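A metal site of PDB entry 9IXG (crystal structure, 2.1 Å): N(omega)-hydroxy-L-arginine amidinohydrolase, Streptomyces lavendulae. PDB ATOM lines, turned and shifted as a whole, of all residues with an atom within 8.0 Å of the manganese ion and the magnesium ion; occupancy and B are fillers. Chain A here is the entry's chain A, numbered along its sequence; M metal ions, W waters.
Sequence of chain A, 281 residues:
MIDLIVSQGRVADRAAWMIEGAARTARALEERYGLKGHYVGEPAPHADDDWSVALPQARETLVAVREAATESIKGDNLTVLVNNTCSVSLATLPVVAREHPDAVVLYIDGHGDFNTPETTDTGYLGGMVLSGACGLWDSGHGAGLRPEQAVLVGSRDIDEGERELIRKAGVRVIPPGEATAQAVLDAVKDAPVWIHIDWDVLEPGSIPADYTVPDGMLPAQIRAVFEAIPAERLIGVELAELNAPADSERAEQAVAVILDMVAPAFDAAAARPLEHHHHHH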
ATOM      1  N   THR A  85      11.182 -19.655   0.950  1.00  0.00           N
ATOM      2  CA  THR A  85      10.238 -19.016   0.039  1.00  0.00           C
ATOM      3  C   THR A  85       9.381 -20.062  -0.643  1.00  0.00           C
ATOM      4  O   THR A  85       9.772 -21.224  -0.762  1.00  0.00           O
ATOM      5  CB  THR A  85      10.934 -18.179  -1.061  1.00  0.00           C
ATOM      6  OG1 THR A  85      11.625 -19.057  -1.962  1.00  0.00           O
ATOM      7  CG2 THR A  85      11.939 -17.203  -0.446  1.00  0.00           C
ATOM      8  N   CYS A  86       8.213 -19.637  -1.110  1.00  0.00           N
ATOM      9  CA  CYS A  86       7.365 -20.534  -1.883  1.00  0.00           C
ATOM     10  C   CYS A  86       8.072 -21.077  -3.128  1.00  0.00           C
ATOM     11  O   CYS A  86       7.703 -22.147  -3.621  1.00  0.00           O
ATOM     12  CB  CYS A  86       6.070 -19.811  -2.293  1.00  0.00           C
ATOM     13  SG  CYS A  86       4.846 -19.531  -0.972  1.00  0.00           S
ATOM     14  N   SER A  87       9.078 -20.361  -3.644  1.00  0.00           N
ATOM     15  CA  SER A  87       9.732 -20.797  -4.895  1.00  0.00           C
ATOM     16  C   SER A  87      10.458 -22.124  -4.745  1.00  0.00           C
ATOM     17  O   SER A  87      10.732 -22.766  -5.756  1.00  0.00           O
ATOM     18  CB  SER A  87      10.752 -19.737  -5.371  1.00  0.00           C
ATOM     19  OG  SER A  87      10.128 -18.523  -5.654  1.00  0.00           O
ATOM     20  N   TYR A 107      -2.904 -25.184  -1.936  1.00  0.00           N
ATOM     21  CA  TYR A 107      -1.930 -24.087  -1.990  1.00  0.00           C
ATOM     22  C   TYR A 107      -2.532 -22.954  -1.177  1.00  0.00           C
ATOM     23  O   TYR A 107      -3.358 -22.177  -1.679  1.00  0.00           O
ATOM     24  CB  TYR A 107      -1.641 -23.664  -3.427  1.00  0.00           C
ATOM     25  CG  TYR A 107      -0.341 -22.901  -3.623  1.00  0.00           C
ATOM     26  CD1 TYR A 107      -0.284 -21.520  -3.431  1.00  0.00           C
ATOM     27  CD2 TYR A 107       0.819 -23.561  -4.007  1.00  0.00           C
ATOM     28  CE1 TYR A 107       0.895 -20.825  -3.621  1.00  0.00           C
ATOM     29  CE2 TYR A 107       2.011 -22.873  -4.212  1.00  0.00           C
ATOM     30  CZ  TYR A 107       2.040 -21.505  -4.009  1.00  0.00           C
ATOM     31  OH  TYR A 107       3.204 -20.807  -4.212  1.00  0.00           O
ATOM     32  N   ILE A 108      -2.141 -22.865   0.090  1.00  0.00           N
ATOM     33  CA  ILE A 108      -2.749 -21.953   1.044  1.00  0.00           C
ATOM     34  C   ILE A 108      -1.892 -20.700   1.033  1.00  0.00           C
ATOM     35  O   ILE A 108      -0.733 -20.727   1.432  1.00  0.00           O
ATOM     36  CB  ILE A 108      -2.821 -22.599   2.436  1.00  0.00           C
ATOM     37  CG1 ILE A 108      -3.441 -24.008   2.325  1.00  0.00           C
ATOM     38  CG2 ILE A 108      -3.582 -21.710   3.457  1.00  0.00           C
ATOM     39  CD1 ILE A 108      -3.820 -24.635   3.645  1.00  0.00           C
ATOM     40  N   ASP A 109      -2.462 -19.599   0.549  1.00  0.00           N
ATOM     41  CA  ASP A 109      -1.635 -18.422   0.287  1.00  0.00           C
ATOM     42  C   ASP A 109      -2.540 -17.201   0.195  1.00  0.00           C
ATOM     43  O   ASP A 109      -3.652 -17.299  -0.313  1.00  0.00           O
ATOM     44  CB  ASP A 109      -0.878 -18.620  -1.041  1.00  0.00           C
ATOM     45  CG  ASP A 109       0.291 -17.675  -1.217  1.00  0.00           C
ATOM     46  OD1 ASP A 109       0.180 -16.456  -0.980  1.00  0.00           O
ATOM     47  OD2 ASP A 109       1.360 -18.183  -1.602  1.00  0.00           O
ATOM     48  N   GLY A 110      -2.059 -16.063   0.690  1.00  0.00           N
ATOM     49  CA  GLY A 110      -2.796 -14.831   0.456  1.00  0.00           C
ATOM     50  C   GLY A 110      -2.874 -14.455  -1.007  1.00  0.00           C
ATOM     51  O   GLY A 110      -3.751 -13.666  -1.410  1.00  0.00           O
ATOM     52  N   HIS A 111      -1.974 -15.006  -1.826  1.00  0.00           N
ATOM     53  CA  HIS A 111      -1.810 -14.690  -3.233  1.00  0.00           C
ATOM     54  C   HIS A 111      -2.135 -15.914  -4.086  1.00  0.00           C
ATOM     55  O   HIS A 111      -2.210 -17.053  -3.601  1.00  0.00           O
ATOM     56  CB  HIS A 111      -0.371 -14.239  -3.546  1.00  0.00           C
ATOM     57  CG  HIS A 111       0.100 -13.093  -2.703  1.00  0.00           C
ATOM     58  ND1 HIS A 111       0.738 -13.272  -1.495  1.00  0.00           N
ATOM     59  CD2 HIS A 111       0.122 -11.753  -2.953  1.00  0.00           C
ATOM     60  CE1 HIS A 111       1.080 -12.084  -1.003  1.00  0.00           C
ATOM     61  NE2 HIS A 111       0.725 -11.157  -1.869  1.00  0.00           N
ATOM     62  N   GLY A 112      -2.252 -15.671  -5.395  1.00  0.00           N
ATOM     63  CA  GLY A 112      -2.433 -16.766  -6.337  1.00  0.00           C
ATOM     64  C   GLY A 112      -1.143 -17.489  -6.725  1.00  0.00           C
ATOM     65  O   GLY A 112      -1.194 -18.675  -7.080  1.00  0.00           O
ATOM     66  N   ASP A 113       0.002 -16.792  -6.660  1.00  0.00           N
ATOM     67  CA  ASP A 113       1.307 -17.242  -7.158  1.00  0.00           C
ATOM     68  C   ASP A 113       1.210 -17.918  -8.522  1.00  0.00           C
ATOM     69  O   ASP A 113       1.872 -18.920  -8.795  1.00  0.00           O
ATOM     70  CB  ASP A 113       1.996 -18.179  -6.144  1.00  0.00           C
ATOM     71  CG  ASP A 113       2.401 -17.473  -4.843  1.00  0.00           C
ATOM     72  OD1 ASP A 113       2.115 -16.262  -4.688  1.00  0.00           O
ATOM     73  OD2 ASP A 113       3.007 -18.132  -3.967  1.00  0.00           O
ATOM     74  N   TYR A 124       8.986 -11.242  -9.846  1.00  0.00           N
ATOM     75  CA  TYR A 124       9.331 -12.021  -8.657  1.00  0.00           C
ATOM     76  C   TYR A 124       8.988 -13.494  -8.866  1.00  0.00           C
ATOM     77  O   TYR A 124       7.820 -13.844  -9.085  1.00  0.00           O
ATOM     78  CB  TYR A 124       8.597 -11.458  -7.437  1.00  0.00           C
ATOM     79  CG  TYR A 124       8.835 -12.231  -6.164  1.00  0.00           C
ATOM     80  CD1 TYR A 124      10.126 -12.631  -5.803  1.00  0.00           C
ATOM     81  CD2 TYR A 124       7.787 -12.557  -5.334  1.00  0.00           C
ATOM     82  CE1 TYR A 124      10.356 -13.340  -4.623  1.00  0.00           C
ATOM     83  CE2 TYR A 124       7.998 -13.293  -4.156  1.00  0.00           C
ATOM     84  CZ  TYR A 124       9.285 -13.663  -3.797  1.00  0.00           C
ATOM     85  OH  TYR A 124       9.497 -14.388  -2.646  1.00  0.00           O
ATOM     86  N   LEU A 125      10.004 -14.364  -8.787  1.00  0.00           N
ATOM     87  CA  LEU A 125       9.799 -15.813  -8.959  1.00  0.00           C
ATOM     88  C   LEU A 125       8.756 -16.382  -7.988  1.00  0.00           C
ATOM     89  O   LEU A 125       8.052 -17.341  -8.327  1.00  0.00           O
ATOM     90  CB  LEU A 125      11.145 -16.537  -8.777  1.00  0.00           C
ATOM     91  CG  LEU A 125      11.204 -18.045  -9.061  1.00  0.00           C
ATOM     92  CD1 LEU A 125      11.001 -18.318 -10.568  1.00  0.00           C
ATOM     93  CD2 LEU A 125      12.510 -18.670  -8.537  1.00  0.00           C
ATOM     94  N   GLY A 126       8.634 -15.813  -6.774  1.00  0.00           N
ATOM     95  CA  GLY A 126       7.668 -16.338  -5.814  1.00  0.00           C
ATOM     96  C   GLY A 126       6.210 -16.155  -6.201  1.00  0.00           C
ATOM     97  O   GLY A 126       5.337 -16.831  -5.653  1.00  0.00           O
ATOM     98  N   GLY A 127       5.921 -15.226  -7.121  1.00  0.00           N
ATOM     99  CA  GLY A 127       4.621 -15.064  -7.721  1.00  0.00           C
ATOM    100  C   GLY A 127       4.352 -15.957  -8.917  1.00  0.00           C
ATOM    101  O   GLY A 127       3.307 -15.835  -9.557  1.00  0.00           O
ATOM    102  N   MET A 128       5.265 -16.884  -9.227  1.00  0.00           N
ATOM    103  CA  MET A 128       5.168 -17.723 -10.412  1.00  0.00           C
ATOM    104  C   MET A 128       5.260 -19.212 -10.098  1.00  0.00           C
ATOM    105  O   MET A 128       5.538 -20.006 -11.003  1.00  0.00           O
ATOM    106  CB  MET A 128       6.260 -17.356 -11.454  1.00  0.00           C
ATOM    107  CG  MET A 128       6.454 -15.837 -11.764  1.00  0.00           C
ATOM    108  SD  MET A 128       8.059 -15.313 -12.554  1.00  0.00           S
ATOM    109  CE  MET A 128       7.900 -16.141 -14.125  1.00  0.00           C
ATOM    110  N   VAL A 129       4.992 -19.612  -8.837  1.00  0.00           N
ATOM    111  CA  VAL A 129       5.308 -20.960  -8.356  1.00  0.00           C
ATOM    112  C   VAL A 129       4.276 -21.984  -8.822  1.00  0.00           C
ATOM    113  O   VAL A 129       4.619 -23.027  -9.388  1.00  0.00           O
ATOM    114  CB  VAL A 129       5.427 -20.964  -6.815  1.00  0.00           C
ATOM    115  CG1 VAL A 129       5.514 -22.415  -6.267  1.00  0.00           C
ATOM    116  CG2 VAL A 129       6.608 -20.146  -6.363  1.00  0.00           C
ATOM    117  N   LEU A 130       3.012 -21.724  -8.530  1.00  0.00           N
ATOM    118  CA  LEU A 130       1.952 -22.687  -8.851  1.00  0.00           C
ATOM    119  C   LEU A 130       1.707 -22.779 -10.342  1.00  0.00           C
ATOM    120  O   LEU A 130       1.367 -23.848 -10.865  1.00  0.00           O
ATOM    121  CB  LEU A 130       0.668 -22.307  -8.129  1.00  0.00           C
ATOM    122  CG  LEU A 130      -0.529 -23.261  -8.277  1.00  0.00           C
ATOM    123  CD1 LEU A 130      -0.134 -24.662  -7.831  1.00  0.00           C
ATOM    124  CD2 LEU A 130      -1.695 -22.758  -7.443  1.00  0.00           C
ATOM    125  N   LEU A 152      -6.367 -23.177  -4.619  1.00  0.00           N
ATOM    126  CA  LEU A 152      -5.911 -22.024  -3.860  1.00  0.00           C
ATOM    127  C   LEU A 152      -6.834 -21.789  -2.673  1.00  0.00           C
ATOM    128  O   LEU A 152      -8.059 -21.698  -2.827  1.00  0.00           O
ATOM    129  CB  LEU A 152      -5.859 -20.774  -4.747  1.00  0.00           C
ATOM    130  CG  LEU A 152      -4.618 -20.694  -5.648  1.00  0.00           C
ATOM    131  CD1 LEU A 152      -4.849 -19.708  -6.804  1.00  0.00           C
ATOM    132  CD2 LEU A 152      -3.363 -20.324  -4.828  1.00  0.00           C
ATOM    133  N   SER A 155      -6.763 -17.237  -0.887  1.00  0.00           N
ATOM    134  CA  SER A 155      -6.323 -16.151  -1.749  1.00  0.00           C
ATOM    135  C   SER A 155      -7.407 -15.093  -1.887  1.00  0.00           C
ATOM    136  O   SER A 155      -8.604 -15.388  -1.873  1.00  0.00           O
ATOM    137  CB  SER A 155      -5.949 -16.692  -3.131  1.00  0.00           C
ATOM    138  OG  SER A 155      -5.291 -17.923  -3.004  1.00  0.00           O
ATOM    139  N   HIS A 196       0.596 -26.903   1.014  1.00  0.00           N
ATOM    140  CA  HIS A 196       1.632 -25.895   0.888  1.00  0.00           C
ATOM    141  C   HIS A 196       1.092 -24.643   1.579  1.00  0.00           C
ATOM    142  O   HIS A 196       0.024 -24.156   1.212  1.00  0.00           O
ATOM    143  CB  HIS A 196       1.946 -25.669  -0.594  1.00  0.00           C
ATOM    144  CG  HIS A 196       2.729 -24.421  -0.866  1.00  0.00           C
ATOM    145  ND1 HIS A 196       4.032 -24.440  -1.315  1.00  0.00           N
ATOM    146  CD2 HIS A 196       2.398 -23.117  -0.730  1.00  0.00           C
ATOM    147  CE1 HIS A 196       4.472 -23.202  -1.438  1.00  0.00           C
ATOM    148  NE2 HIS A 196       3.493 -22.374  -1.098  1.00  0.00           N
ATOM    149  N   ILE A 197       1.804 -24.132   2.587  1.00  0.00           N
ATOM    150  CA  ILE A 197       1.373 -22.912   3.274  1.00  0.00           C
ATOM    151  C   ILE A 197       2.368 -21.774   3.076  1.00  0.00           C
ATOM    152  O   ILE A 197       3.550 -21.920   3.393  1.00  0.00           O
ATOM    153  CB  ILE A 197       1.152 -23.128   4.778  1.00  0.00           C
ATOM    154  CG1 ILE A 197       0.418 -24.442   5.027  1.00  0.00           C
ATOM    155  CG2 ILE A 197       0.405 -21.930   5.334  1.00  0.00           C
ATOM    156  CD1 ILE A 197      -0.144 -24.546   6.430  1.00  0.00           C
ATOM    157  N   ASP A 198       1.864 -20.615   2.640  1.00  0.00           N
ATOM    158  CA  ASP A 198       2.523 -19.314   2.685  1.00  0.00           C
ATOM    159  C   ASP A 198       1.877 -18.532   3.822  1.00  0.00           C
ATOM    160  O   ASP A 198       0.674 -18.258   3.778  1.00  0.00           O
ATOM    161  CB  ASP A 198       2.332 -18.618   1.315  1.00  0.00           C
ATOM    162  CG  ASP A 198       2.992 -17.224   1.207  1.00  0.00           C
ATOM    163  OD1 ASP A 198       3.356 -16.611   2.235  1.00  0.00           O
ATOM    164  OD2 ASP A 198       3.086 -16.706   0.038  1.00  0.00           O
ATOM    165  N   TRP A 199       2.659 -18.175   4.852  1.00  0.00           N
ATOM    166  CA  TRP A 199       2.076 -17.520   6.025  1.00  0.00           C
ATOM    167  C   TRP A 199       1.485 -16.120   5.724  1.00  0.00           C
ATOM    168  O   TRP A 199       0.733 -15.615   6.567  1.00  0.00           O
ATOM    169  CB  TRP A 199       3.116 -17.411   7.165  1.00  0.00           C
ATOM    170  CG  TRP A 199       3.629 -18.770   7.630  1.00  0.00           C
ATOM    171  CD1 TRP A 199       4.932 -19.196   7.666  1.00  0.00           C
ATOM    172  CD2 TRP A 199       2.836 -19.881   8.107  1.00  0.00           C
ATOM    173  NE1 TRP A 199       5.011 -20.488   8.115  1.00  0.00           N
ATOM    174  CE2 TRP A 199       3.741 -20.939   8.415  1.00  0.00           C
ATOM    175  CE3 TRP A 199       1.474 -20.082   8.329  1.00  0.00           C
ATOM    176  CZ2 TRP A 199       3.310 -22.179   8.893  1.00  0.00           C
ATOM    177  CZ3 TRP A 199       1.044 -21.322   8.807  1.00  0.00           C
ATOM    178  CH2 TRP A 199       1.970 -22.342   9.088  1.00  0.00           C
ATOM    179  N   ASP A 200       1.751 -15.512   4.560  1.00  0.00           N
ATOM    180  CA  ASP A 200       1.011 -14.262   4.303  1.00  0.00           C
ATOM    181  C   ASP A 200      -0.500 -14.476   4.122  1.00  0.00           C
ATOM    182  O   ASP A 200      -1.246 -13.493   4.025  1.00  0.00           O
ATOM    183  CB  ASP A 200       1.618 -13.472   3.094  1.00  0.00           C
ATOM    184  CG  ASP A 200       1.519 -14.189   1.707  1.00  0.00           C
ATOM    185  OD1 ASP A 200       0.533 -14.893   1.431  1.00  0.00           O
ATOM    186  OD2 ASP A 200       2.447 -13.991   0.853  1.00  0.00           O
ATOM    187  N   VAL A 201      -0.979 -15.731   4.136  1.00  0.00           N
ATOM    188  CA  VAL A 201      -2.419 -15.979   4.092  1.00  0.00           C
ATOM    189  C   VAL A 201      -3.112 -15.485   5.368  1.00  0.00           C
ATOM    190  O   VAL A 201      -4.297 -15.150   5.334  1.00  0.00           O
ATOM    191  CB  VAL A 201      -2.693 -17.491   3.859  1.00  0.00           C
ATOM    192  CG1 VAL A 201      -2.376 -18.326   5.108  1.00  0.00           C
ATOM    193  CG2 VAL A 201      -4.141 -17.729   3.402  1.00  0.00           C
ATOM    194  N   ALA A 240       6.207 -22.187   4.402  1.00  0.00           N
ATOM    195  CA  ALA A 240       7.069 -21.227   3.729  1.00  0.00           C
ATOM    196  C   ALA A 240       6.770 -19.804   4.169  1.00  0.00           C
ATOM    197  O   ALA A 240       5.636 -19.461   4.492  1.00  0.00           O
ATOM    198  CB  ALA A 240       6.934 -21.317   2.198  1.00  0.00           C
ATOM    199  N   GLU A 241       7.826 -18.972   4.154  1.00  0.00           N
ATOM    200  CA  GLU A 241       7.739 -17.503   4.180  1.00  0.00           C
ATOM    201  C   GLU A 241       7.352 -16.945   5.550  1.00  0.00           C
ATOM    202  O   GLU A 241       6.532 -16.029   5.674  1.00  0.00           O
ATOM    203  CB  GLU A 241       6.789 -16.999   3.068  1.00  0.00           C
ATOM    204  CG  GLU A 241       7.217 -17.539   1.690  1.00  0.00           C
ATOM    205  CD  GLU A 241       7.056 -16.570   0.501  1.00  0.00           C
ATOM    206  OE1 GLU A 241       6.555 -15.433   0.671  1.00  0.00           O
ATOM    207  OE2 GLU A 241       7.408 -16.974  -0.619  1.00  0.00           O
HETATM  208 MN    MN M   1       3.421 -17.540  -1.871  1.00  0.00          MN
HETATM  209 MG    MG M   2       1.623 -15.028  -0.607  1.00  0.00          MG
HETATM  210  O   HOH W   1       2.764 -15.541  -2.307  1.00  0.00           O
HETATM  211  O   HOH W   2       5.224 -16.524  -2.424  1.00  0.00           O
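OD2 of Asp 200 binds the magnesium ion, at 2.0 Å. OD1 of Asp 109 binds the magnesium ion. The magnesium ion is bound by water W1 (2.1 Å). The magnesium ion is bound by ND1 of His 111 (2.2 Å). OD1 of Asp 200 binds the magnesium ion. The magnesium ion is bound by OD2 of Asp 198, at 2.3 Å.
The manganese ion is bound by OD2 of Asp 198 (2.1 Å), water W2 (2.1 Å), water W1 (2.1 Å), OD2 of Asp 109 (2.2 Å), OD2 of Asp 113 (2.2 Å) and SG of Cys 86 (2.6 Å). The manganese ion has six donor atoms within binding distance.
The side-chain carboxylate of Asp 200 lies close to the backbone NH of Gly 110 (2.9 Å). The backbone carbonyl oxygen of Asp 109 is in hydrogen-bond range of the backbone NH of Ser 155 (3.2 Å). The backbone carbonyl oxygen of Ile 108 sits at hydrogen-bond distance from the backbone NH of Asp 198 (2.9 Å). The side-chain hydroxyl (OG) of Ser 155 sits at hydrogen-bond distance from the backbone carbonyl oxygen (O) of His 111, at 3.3 Å. The side-chain carboxylate (OD2) of Asp 113 sits close to the side-chain hydroxyl (OH) of Tyr 107 (2.7 Å). O of Asp 113 lies within hydrogen-bond range of N of Val 129 (3.2 Å). O of Asp 113 is in hydrogen-bond range of N of Leu 130 (3.0 Å). OE2 of Glu 241 lies within hydrogen-bond range of N of Cys 86 (2.8 Å).
Within 4 Å of the magnesium ion: Asp 109, His 111, Asp 198 and Asp 200.
Of the 27 residues printed, 4 come within 4 Å of the manganese ion.
Water W2 lies within hydrogen-bond range of the side-chain carboxylate of Glu 241 (2.9 Å) and the backbone carbonyl oxygen of Gly 126 (3.2 Å).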
